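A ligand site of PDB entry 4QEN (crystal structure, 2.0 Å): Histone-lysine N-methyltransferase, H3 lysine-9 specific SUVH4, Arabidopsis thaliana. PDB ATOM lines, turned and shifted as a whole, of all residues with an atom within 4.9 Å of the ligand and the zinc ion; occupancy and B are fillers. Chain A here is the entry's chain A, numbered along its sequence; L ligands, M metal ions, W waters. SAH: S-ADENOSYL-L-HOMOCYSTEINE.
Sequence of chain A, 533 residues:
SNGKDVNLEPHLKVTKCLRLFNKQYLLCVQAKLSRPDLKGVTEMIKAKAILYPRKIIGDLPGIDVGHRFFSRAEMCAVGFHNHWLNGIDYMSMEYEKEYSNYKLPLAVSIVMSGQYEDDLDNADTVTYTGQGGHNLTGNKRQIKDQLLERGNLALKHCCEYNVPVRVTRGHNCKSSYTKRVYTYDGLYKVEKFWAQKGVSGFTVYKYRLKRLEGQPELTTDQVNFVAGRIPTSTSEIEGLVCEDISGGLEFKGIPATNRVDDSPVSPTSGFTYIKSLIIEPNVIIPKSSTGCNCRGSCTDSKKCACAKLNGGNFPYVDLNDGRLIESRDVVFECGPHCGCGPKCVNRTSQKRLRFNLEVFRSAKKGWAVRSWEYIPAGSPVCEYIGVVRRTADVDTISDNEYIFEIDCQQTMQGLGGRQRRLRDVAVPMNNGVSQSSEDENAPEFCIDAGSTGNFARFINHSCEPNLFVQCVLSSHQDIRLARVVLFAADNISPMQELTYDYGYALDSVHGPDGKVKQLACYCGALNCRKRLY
The zinc ion is bound by SG of Cys 521, SG of Cys 523, SG of Cys 528 and SG of Cys 463.
SD of the ligand sits close to O of Glu 401, 3.6 Å away. The backbone carbonyl oxygen (O) of Arg 457 sits close to a sulfur (SD) of the ligand (3.5 Å). Merely in contact with the ligand: Tyr 502 (3.3 Å), Ala 520 (3.4 Å), Gly 366 (3.4 Å), Leu 532 (3.4 Å), Ile 459 (3.7 Å) and Phe 458 (3.8 Å). Hydrophobic or aromatic side chains that line the ligand: Trp 367, Tyr 402, His 461, Tyr 502, Tyr 522 and Leu 532. 16 residues have an atom within 4 Å of the ligand: Lys 365, Gly 366, Trp 367, Glu 401, Tyr 402, Arg 457, Phe 458, Ile 459, Asn 460, His 461, Tyr 502, Ala 520, Cys 521, Tyr 522, Cys 523 and Leu 532.
N of Cys 521 lies within hydrogen-bond range of O of Lys 530. The side-chain sulfur (SG) of Cys 523 sits close to the side-chain hydroxyl (OG) of Ser 462, at 3.7 Å. The side-chain sulfur (SG) of Cys 528 sits close to the backbone NH (N) of Lys 530, at 3.4 Å. A ring nitrogen (NE2) of His 461 lies close to the side-chain sulfur of Cys 463 (3.5 Å). The backbone carbonyl oxygen (O) of Trp 367 lies within hydrogen-bond range of the side-chain amide nitrogen (ND2) of Asn 460 (3.0 Å). ND1 of His 461 lies within hydrogen-bond range of N of Tyr 502 (2.9 Å). OH of Tyr 502 is in hydrogen-bond range of O of Ile 459, at 2.8 Å. O of Leu 519 sits at hydrogen-bond distance from N of Leu 532 (2.8 Å).
Along chain A the residues within 4 Å of the zinc ion span positions 463 to 528.
The side-chain sulfur (SG) of Cys 521 sits close to a nitrogen (N6) of the ligand (3.4 Å). OXT of the ligand lies within hydrogen-bond range of N of Trp 367 (2.5 Å). The backbone carbonyl oxygen (O) of Trp 367 sits at hydrogen-bond distance from a nitrogen (N) of the ligand. O of Lys 365 is in hydrogen-bond range of N of the ligand (2.6 Å). OH of Tyr 402 lies within hydrogen-bond range of O of the ligand, 2.6 Å away. A nitrogen (N) of the ligand sits at hydrogen-bond distance from the side-chain amide oxygen of Asn 460 (2.7 Å). N of His 461 is in hydrogen-bond range of N7 of the ligand, 3.0 Å away. The backbone carbonyl oxygen of His 461 is in hydrogen-bond range of a nitrogen (N6) of the ligand (2.8 Å). N of Tyr 522 sits at hydrogen-bond distance from N1 of the ligand, at 2.9 Å.
Water W2 bridges NH2 of Arg 361 and OXT of the ligand.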
ATOM      1  N   ARG A 361     -13.409 -14.991  -3.798  1.00  0.00           N
ATOM      2  CA  ARG A 361     -13.460 -15.915  -2.662  1.00  0.00           C
ATOM      3  C   ARG A 361     -12.310 -16.902  -2.682  1.00  0.00           C
ATOM      4  O   ARG A 361     -12.216 -17.723  -3.595  1.00  0.00           O
ATOM      5  CB  ARG A 361     -14.778 -16.710  -2.677  1.00  0.00           C
ATOM      6  CG  ARG A 361     -15.715 -16.391  -1.522  1.00  0.00           C
ATOM      7  CD  ARG A 361     -15.153 -16.758  -0.160  1.00  0.00           C
ATOM      8  NE  ARG A 361     -15.548 -15.779   0.840  1.00  0.00           N
ATOM      9  CZ  ARG A 361     -15.840 -16.048   2.107  1.00  0.00           C
ATOM     10  NH1 ARG A 361     -15.779 -17.295   2.550  1.00  0.00           N
ATOM     11  NH2 ARG A 361     -16.193 -15.075   2.924  1.00  0.00           N
ATOM     12  N   LYS A 364      -9.760 -20.765   1.840  1.00  0.00           N
ATOM     13  CA  LYS A 364      -9.653 -20.870   3.303  1.00  0.00           C
ATOM     14  C   LYS A 364      -9.346 -19.559   4.016  1.00  0.00           C
ATOM     15  O   LYS A 364      -9.210 -19.541   5.227  1.00  0.00           O
ATOM     16  CB  LYS A 364      -8.603 -21.919   3.679  1.00  0.00           C
ATOM     17  CG  LYS A 364      -8.982 -23.365   3.364  1.00  0.00           C
ATOM     18  CD  LYS A 364      -9.961 -23.945   4.388  1.00  0.00           C
ATOM     19  CE  LYS A 364     -10.538 -25.258   3.890  1.00  0.00           C
ATOM     20  NZ  LYS A 364     -11.430 -25.934   4.875  1.00  0.00           N
ATOM     21  N   LYS A 365      -9.248 -18.462   3.273  1.00  0.00           N
ATOM     22  CA  LYS A 365      -8.884 -17.189   3.889  1.00  0.00           C
ATOM     23  C   LYS A 365     -10.018 -16.179   3.805  1.00  0.00           C
ATOM     24  O   LYS A 365      -9.871 -15.040   4.228  1.00  0.00           O
ATOM     25  CB  LYS A 365      -7.615 -16.606   3.244  1.00  0.00           C
ATOM     26  CG  LYS A 365      -6.440 -17.595   3.173  1.00  0.00           C
ATOM     27  CD  LYS A 365      -5.227 -17.011   2.453  1.00  0.00           C
ATOM     28  CE  LYS A 365      -5.544 -16.687   1.002  1.00  0.00           C
ATOM     29  NZ  LYS A 365      -4.301 -16.433   0.211  1.00  0.00           N
ATOM     30  N   GLY A 366     -11.158 -16.602   3.259  1.00  0.00           N
ATOM     31  CA  GLY A 366     -12.273 -15.693   3.024  1.00  0.00           C
ATOM     32  C   GLY A 366     -12.018 -14.878   1.773  1.00  0.00           C
ATOM     33  O   GLY A 366     -11.398 -15.379   0.835  1.00  0.00           O
ATOM     34  N   TRP A 367     -12.449 -13.614   1.754  1.00  0.00           N
ATOM     35  CA  TRP A 367     -12.256 -12.769   0.581  1.00  0.00           C
ATOM     36  C   TRP A 367     -10.778 -12.421   0.383  1.00  0.00           C
ATOM     37  O   TRP A 367     -10.001 -12.397   1.348  1.00  0.00           O
ATOM     38  CB  TRP A 367     -13.079 -11.482   0.660  1.00  0.00           C
ATOM     39  CG  TRP A 367     -14.564 -11.689   0.737  1.00  0.00           C
ATOM     40  CD1 TRP A 367     -15.369 -11.497   1.829  1.00  0.00           C
ATOM     41  CD2 TRP A 367     -15.426 -12.134  -0.319  1.00  0.00           C
ATOM     42  NE1 TRP A 367     -16.677 -11.794   1.509  1.00  0.00           N
ATOM     43  CE2 TRP A 367     -16.741 -12.185   0.204  1.00  0.00           C
ATOM     44  CE3 TRP A 367     -15.217 -12.497  -1.657  1.00  0.00           C
ATOM     45  CZ2 TRP A 367     -17.831 -12.589  -0.564  1.00  0.00           C
ATOM     46  CZ3 TRP A 367     -16.311 -12.877  -2.420  1.00  0.00           C
ATOM     47  CH2 TRP A 367     -17.602 -12.932  -1.877  1.00  0.00           C
ATOM     48  N   GLU A 401     -11.557  -8.204  12.907  1.00  0.00           N
ATOM     49  CA  GLU A 401     -10.420  -8.606  12.067  1.00  0.00           C
ATOM     50  C   GLU A 401      -9.992  -7.553  11.046  1.00  0.00           C
ATOM     51  O   GLU A 401      -9.197  -7.837  10.151  1.00  0.00           O
ATOM     52  CB  GLU A 401     -10.754  -9.903  11.325  1.00  0.00           C
ATOM     53  CG  GLU A 401     -11.197 -11.055  12.217  1.00  0.00           C
ATOM     54  CD  GLU A 401     -11.768 -12.215  11.421  1.00  0.00           C
ATOM     55  OE1 GLU A 401     -12.090 -12.026  10.235  1.00  0.00           O
ATOM     56  OE2 GLU A 401     -11.888 -13.318  11.989  1.00  0.00           O
ATOM     57  N   TYR A 402     -10.518  -6.334  11.172  1.00  0.00           N
ATOM     58  CA  TYR A 402     -10.278  -5.322  10.148  1.00  0.00           C
ATOM     59  C   TYR A 402      -9.654  -4.047  10.687  1.00  0.00           C
ATOM     60  O   TYR A 402      -9.826  -2.969  10.119  1.00  0.00           O
ATOM     61  CB  TYR A 402     -11.579  -4.997   9.403  1.00  0.00           C
ATOM     62  CG  TYR A 402     -12.218  -6.196   8.750  1.00  0.00           C
ATOM     63  CD1 TYR A 402     -11.783  -6.651   7.504  1.00  0.00           C
ATOM     64  CD2 TYR A 402     -13.261  -6.894   9.370  1.00  0.00           C
ATOM     65  CE1 TYR A 402     -12.352  -7.737   6.887  1.00  0.00           C
ATOM     66  CE2 TYR A 402     -13.846  -7.998   8.769  1.00  0.00           C
ATOM     67  CZ  TYR A 402     -13.383  -8.412   7.528  1.00  0.00           C
ATOM     68  OH  TYR A 402     -13.957  -9.511   6.909  1.00  0.00           O
ATOM     69  N   ARG A 457      -9.188  -3.490   3.178  1.00  0.00           N
ATOM     70  CA  ARG A 457      -9.575  -4.445   4.206  1.00  0.00           C
ATOM     71  C   ARG A 457      -9.756  -5.872   3.640  1.00  0.00           C
ATOM     72  O   ARG A 457      -9.893  -6.819   4.404  1.00  0.00           O
ATOM     73  CB  ARG A 457     -10.897  -3.996   4.833  1.00  0.00           C
ATOM     74  CG  ARG A 457     -12.041  -4.399   3.936  1.00  0.00           C
ATOM     75  CD  ARG A 457     -13.347  -3.803   4.287  1.00  0.00           C
ATOM     76  NE  ARG A 457     -13.895  -4.198   5.584  1.00  0.00           N
ATOM     77  CZ  ARG A 457     -14.756  -5.197   5.774  1.00  0.00           C
ATOM     78  NH1 ARG A 457     -15.221  -5.445   6.994  1.00  0.00           N
ATOM     79  NH2 ARG A 457     -15.138  -5.947   4.741  1.00  0.00           N
ATOM     80  N   PHE A 458      -9.800  -6.018   2.324  1.00  0.00           N
ATOM     81  CA  PHE A 458      -9.979  -7.349   1.723  1.00  0.00           C
ATOM     82  C   PHE A 458      -8.667  -8.055   1.380  1.00  0.00           C
ATOM     83  O   PHE A 458      -8.655  -9.217   1.006  1.00  0.00           O
ATOM     84  CB  PHE A 458     -10.909  -7.278   0.503  1.00  0.00           C
ATOM     85  CG  PHE A 458     -12.343  -6.938   0.852  1.00  0.00           C
ATOM     86  CD1 PHE A 458     -13.112  -7.821   1.601  1.00  0.00           C
ATOM     87  CD2 PHE A 458     -12.910  -5.744   0.446  1.00  0.00           C
ATOM     88  CE1 PHE A 458     -14.433  -7.515   1.937  1.00  0.00           C
ATOM     89  CE2 PHE A 458     -14.220  -5.433   0.763  1.00  0.00           C
ATOM     90  CZ  PHE A 458     -14.985  -6.333   1.515  1.00  0.00           C
ATOM     91  N   ILE A 459      -7.555  -7.339   1.535  1.00  0.00           N
ATOM     92  CA  ILE A 459      -6.234  -7.871   1.235  1.00  0.00           C
ATOM     93  C   ILE A 459      -5.714  -8.765   2.375  1.00  0.00           C
ATOM     94  O   ILE A 459      -5.721  -8.366   3.542  1.00  0.00           O
ATOM     95  CB  ILE A 459      -5.247  -6.731   0.951  1.00  0.00           C
ATOM     96  CG1 ILE A 459      -5.799  -5.862  -0.196  1.00  0.00           C
ATOM     97  CG2 ILE A 459      -3.831  -7.259   0.682  1.00  0.00           C
ATOM     98  CD1 ILE A 459      -5.000  -4.556  -0.487  1.00  0.00           C
ATOM     99  N   ASN A 460      -5.268  -9.968   2.019  1.00  0.00           N
ATOM    100  CA  ASN A 460      -4.852 -10.962   3.011  1.00  0.00           C
ATOM    101  C   ASN A 460      -3.381 -10.861   3.407  1.00  0.00           C
ATOM    102  O   ASN A 460      -2.601 -10.157   2.759  1.00  0.00           O
ATOM    103  CB  ASN A 460      -5.143 -12.380   2.525  1.00  0.00           C
ATOM    104  CG  ASN A 460      -6.631 -12.680   2.455  1.00  0.00           C
ATOM    105  OD1 ASN A 460      -7.375 -12.408   3.408  1.00  0.00           O
ATOM    106  ND2 ASN A 460      -7.078 -13.224   1.333  1.00  0.00           N
ATOM    107  N   HIS A 461      -3.030 -11.566   4.477  1.00  0.00           N
ATOM    108  CA  HIS A 461      -1.654 -11.668   4.947  1.00  0.00           C
ATOM    109  C   HIS A 461      -0.879 -12.726   4.178  1.00  0.00           C
ATOM    110  O   HIS A 461      -1.420 -13.788   3.857  1.00  0.00           O
ATOM    111  CB  HIS A 461      -1.639 -12.061   6.427  1.00  0.00           C
ATOM    112  CG  HIS A 461      -0.319 -12.591   6.884  1.00  0.00           C
ATOM    113  ND1 HIS A 461       0.711 -11.777   7.285  1.00  0.00           N
ATOM    114  CD2 HIS A 461       0.149 -13.865   6.986  1.00  0.00           C
ATOM    115  CE1 HIS A 461       1.760 -12.512   7.612  1.00  0.00           C
ATOM    116  NE2 HIS A 461       1.441 -13.785   7.428  1.00  0.00           N
ATOM    117  N   SER A 462       0.391 -12.463   3.906  1.00  0.00           N
ATOM    118  CA  SER A 462       1.303 -13.516   3.487  1.00  0.00           C
ATOM    119  C   SER A 462       2.635 -13.439   4.226  1.00  0.00           C
ATOM    120  O   SER A 462       3.099 -12.350   4.555  1.00  0.00           O
ATOM    121  CB  SER A 462       1.551 -13.481   1.982  1.00  0.00           C
ATOM    122  OG  SER A 462       2.538 -14.448   1.612  1.00  0.00           O
ATOM    123  N   CYS A 463       3.239 -14.589   4.482  1.00  0.00           N
ATOM    124  CA  CYS A 463       4.584 -14.643   5.029  1.00  0.00           C
ATOM    125  C   CYS A 463       5.641 -14.287   3.960  1.00  0.00           C
ATOM    126  O   CYS A 463       6.776 -13.978   4.297  1.00  0.00           O
ATOM    127  CB  CYS A 463       4.849 -16.024   5.643  1.00  0.00           C
ATOM    128  SG  CYS A 463       3.588 -16.520   6.911  1.00  0.00           S
ATOM    129  N   TYR A 502       1.119  -8.990   7.891  1.00  0.00           N
ATOM    130  CA  TYR A 502       0.383  -8.295   8.967  1.00  0.00           C
ATOM    131  C   TYR A 502       1.312  -7.929  10.131  1.00  0.00           C
ATOM    132  O   TYR A 502       1.051  -6.981  10.868  1.00  0.00           O
ATOM    133  CB  TYR A 502      -0.806  -9.113   9.483  1.00  0.00           C
ATOM    134  CG  TYR A 502      -2.005  -9.209   8.565  1.00  0.00           C
ATOM    135  CD1 TYR A 502      -1.991  -8.633   7.287  1.00  0.00           C
ATOM    136  CD2 TYR A 502      -3.156  -9.895   8.958  1.00  0.00           C
ATOM    137  CE1 TYR A 502      -3.091  -8.730   6.435  1.00  0.00           C
ATOM    138  CE2 TYR A 502      -4.254  -9.996   8.123  1.00  0.00           C
ATOM    139  CZ  TYR A 502      -4.216  -9.417   6.872  1.00  0.00           C
ATOM    140  OH  TYR A 502      -5.331  -9.543   6.046  1.00  0.00           O
ATOM    141  N   LEU A 519      -3.883 -18.533  15.459  1.00  0.00           N
ATOM    142  CA  LEU A 519      -4.580 -18.429  14.171  1.00  0.00           C
ATOM    143  C   LEU A 519      -3.688 -18.964  13.052  1.00  0.00           C
ATOM    144  O   LEU A 519      -2.613 -18.430  12.812  1.00  0.00           O
ATOM    145  CB  LEU A 519      -4.945 -16.982  13.859  1.00  0.00           C
ATOM    146  CG  LEU A 519      -6.282 -16.724  13.147  1.00  0.00           C
ATOM    147  CD1 LEU A 519      -6.230 -15.445  12.324  1.00  0.00           C
ATOM    148  CD2 LEU A 519      -6.756 -17.898  12.290  1.00  0.00           C
ATOM    149  N   ALA A 520      -4.150 -19.998  12.367  1.00  0.00           N
ATOM    150  CA  ALA A 520      -3.356 -20.643  11.317  1.00  0.00           C
ATOM    151  C   ALA A 520      -3.184 -19.759  10.076  1.00  0.00           C
ATOM    152  O   ALA A 520      -4.101 -19.026   9.680  1.00  0.00           O
ATOM    153  CB  ALA A 520      -3.982 -21.984  10.937  1.00  0.00           C
ATOM    154  N   CYS A 521      -2.003 -19.797   9.476  1.00  0.00           N
ATOM    155  CA  CYS A 521      -1.772 -19.094   8.219  1.00  0.00           C
ATOM    156  C   CYS A 521      -1.933 -20.031   7.037  1.00  0.00           C
ATOM    157  O   CYS A 521      -1.413 -21.150   7.037  1.00  0.00           O
ATOM    158  CB  CYS A 521      -0.371 -18.477   8.174  1.00  0.00           C
ATOM    159  SG  CYS A 521      -0.127 -17.509   6.680  1.00  0.00           S
ATOM    160  N   TYR A 522      -2.635 -19.564   6.012  1.00  0.00           N
ATOM    161  CA  TYR A 522      -2.828 -20.362   4.807  1.00  0.00           C
ATOM    162  C   TYR A 522      -2.223 -19.686   3.578  1.00  0.00           C
ATOM    163  O   TYR A 522      -2.706 -19.889   2.474  1.00  0.00           O
ATOM    164  CB  TYR A 522      -4.327 -20.598   4.579  1.00  0.00           C
ATOM    165  CG  TYR A 522      -4.928 -21.683   5.437  1.00  0.00           C
ATOM    166  CD1 TYR A 522      -4.972 -23.006   5.004  1.00  0.00           C
ATOM    167  CD2 TYR A 522      -5.458 -21.382   6.683  1.00  0.00           C
ATOM    168  CE1 TYR A 522      -5.532 -23.992   5.798  1.00  0.00           C
ATOM    169  CE2 TYR A 522      -6.011 -22.365   7.489  1.00  0.00           C
ATOM    170  CZ  TYR A 522      -6.046 -23.665   7.035  1.00  0.00           C
ATOM    171  OH  TYR A 522      -6.600 -24.645   7.825  1.00  0.00           O
ATOM    172  N   CYS A 523      -1.182 -18.870   3.771  1.00  0.00           N
ATOM    173  CA  CYS A 523      -0.666 -18.082   2.650  1.00  0.00           C
ATOM    174  C   CYS A 523      -0.022 -18.948   1.576  1.00  0.00           C
ATOM    175  O   CYS A 523       0.179 -18.511   0.445  1.00  0.00           O
ATOM    176  CB  CYS A 523       0.316 -16.992   3.130  1.00  0.00           C
ATOM    177  SG  CYS A 523       1.983 -17.578   3.572  1.00  0.00           S
ATOM    178  N   GLY A 524       0.312 -20.191   1.941  1.00  0.00           N
ATOM    179  CA  GLY A 524       0.832 -21.157   0.994  1.00  0.00           C
ATOM    180  C   GLY A 524       2.288 -20.935   0.610  1.00  0.00           C
ATOM    181  O   GLY A 524       2.815 -21.589  -0.287  1.00  0.00           O
ATOM    182  N   CYS A 528       6.290 -20.528   5.132  1.00  0.00           N
ATOM    183  CA  CYS A 528       5.075 -20.011   5.800  1.00  0.00           C
ATOM    184  C   CYS A 528       5.069 -19.807   7.333  1.00  0.00           C
ATOM    185  O   CYS A 528       4.320 -18.994   7.813  1.00  0.00           O
ATOM    186  CB  CYS A 528       3.837 -20.802   5.375  1.00  0.00           C
ATOM    187  SG  CYS A 528       2.323 -20.322   6.261  1.00  0.00           S
ATOM    188  N   LYS A 530       3.360 -20.711   9.436  1.00  0.00           N
ATOM    189  CA  LYS A 530       2.086 -21.391   9.744  1.00  0.00           C
ATOM    190  C   LYS A 530       1.096 -20.702  10.695  1.00  0.00           C
ATOM    191  O   LYS A 530       0.044 -21.260  10.988  1.00  0.00           O
ATOM    192  CB  LYS A 530       2.343 -22.834  10.223  1.00  0.00           C
ATOM    193  CG  LYS A 530       2.822 -23.764   9.127  1.00  0.00           C
ATOM    194  CD  LYS A 530       1.755 -23.945   8.067  1.00  0.00           C
ATOM    195  CE  LYS A 530       2.251 -24.849   6.963  1.00  0.00           C
ATOM    196  NZ  LYS A 530       2.822 -26.099   7.547  1.00  0.00           N
ATOM    197  N   LEU A 532      -0.686 -16.684  11.695  1.00  0.00           N
ATOM    198  CA  LEU A 532      -0.781 -15.236  11.611  1.00  0.00           C
ATOM    199  C   LEU A 532      -0.330 -14.725  12.958  1.00  0.00           C
ATOM    200  O   LEU A 532       0.365 -13.702  13.065  1.00  0.00           O
ATOM    201  CB  LEU A 532      -2.206 -14.770  11.303  1.00  0.00           C
ATOM    202  CG  LEU A 532      -2.497 -14.345   9.867  1.00  0.00           C
ATOM    203  CD1 LEU A 532      -2.401 -15.554   8.936  1.00  0.00           C
ATOM    204  CD2 LEU A 532      -3.860 -13.685   9.752  1.00  0.00           C
HETATM  205  N   SAH L   1      -9.945 -12.482   4.127  1.00  0.00           N
HETATM  206  CA  SAH L   1     -10.661 -11.399   4.782  1.00  0.00           C
HETATM  207  CB  SAH L   1     -10.033 -10.050   4.436  1.00  0.00           C
HETATM  208  CG  SAH L   1      -8.747  -9.776   5.204  1.00  0.00           C
HETATM  209  SD  SAH L   1      -9.157  -9.213   6.874  1.00  0.00           S
HETATM  210  C   SAH L   1     -12.153 -11.387   4.457  1.00  0.00           C
HETATM  211  O   SAH L   1     -12.828 -10.383   4.679  1.00  0.00           O
HETATM  212  OXT SAH L   1     -12.701 -12.368   3.963  1.00  0.00           O
HETATM  213  C5' SAH L   1      -8.012 -10.338   7.703  1.00  0.00           C
HETATM  214  C4' SAH L   1      -8.639 -11.676   8.081  1.00  0.00           C
HETATM  215  O4' SAH L   1      -8.635 -12.539   6.953  1.00  0.00           O
HETATM  216  C3' SAH L   1      -7.857 -12.361   9.181  1.00  0.00           C
HETATM  217  O3' SAH L   1      -8.408 -12.131  10.452  1.00  0.00           O
HETATM  218  C2' SAH L   1      -7.978 -13.824   8.820  1.00  0.00           C
HETATM  219  O2' SAH L   1      -9.176 -14.347   9.331  1.00  0.00           O
HETATM  220  C1' SAH L   1      -8.097 -13.799   7.308  1.00  0.00           C
HETATM  221  N9  SAH L   1      -6.760 -13.984   6.722  1.00  0.00           N
HETATM  222  C8  SAH L   1      -5.978 -13.025   6.109  1.00  0.00           C
HETATM  223  N7  SAH L   1      -4.815 -13.613   5.711  1.00  0.00           N
HETATM  224  C5  SAH L   1      -4.845 -14.920   6.066  1.00  0.00           C
HETATM  225  C6  SAH L   1      -3.927 -15.965   5.902  1.00  0.00           C
HETATM  226  N6  SAH L   1      -2.760 -15.769   5.299  1.00  0.00           N
HETATM  227  N1  SAH L   1      -4.258 -17.219   6.390  1.00  0.00           N
HETATM  228  C2  SAH L   1      -5.462 -17.442   7.016  1.00  0.00           C
HETATM  229  N3  SAH L   1      -6.365 -16.402   7.171  1.00  0.00           N
HETATM  230  C4  SAH L   1      -6.066 -15.168   6.701  1.00  0.00           C
HETATM  231 ZN    ZN M   1       1.969 -18.022   5.885  1.00  0.00          ZN
HETATM  232  O   HOH W   1      -8.645 -17.440   8.636  1.00  0.00           O
HETATM  233  O   HOH W   2     -15.210 -13.374   4.840  1.00  0.00           O
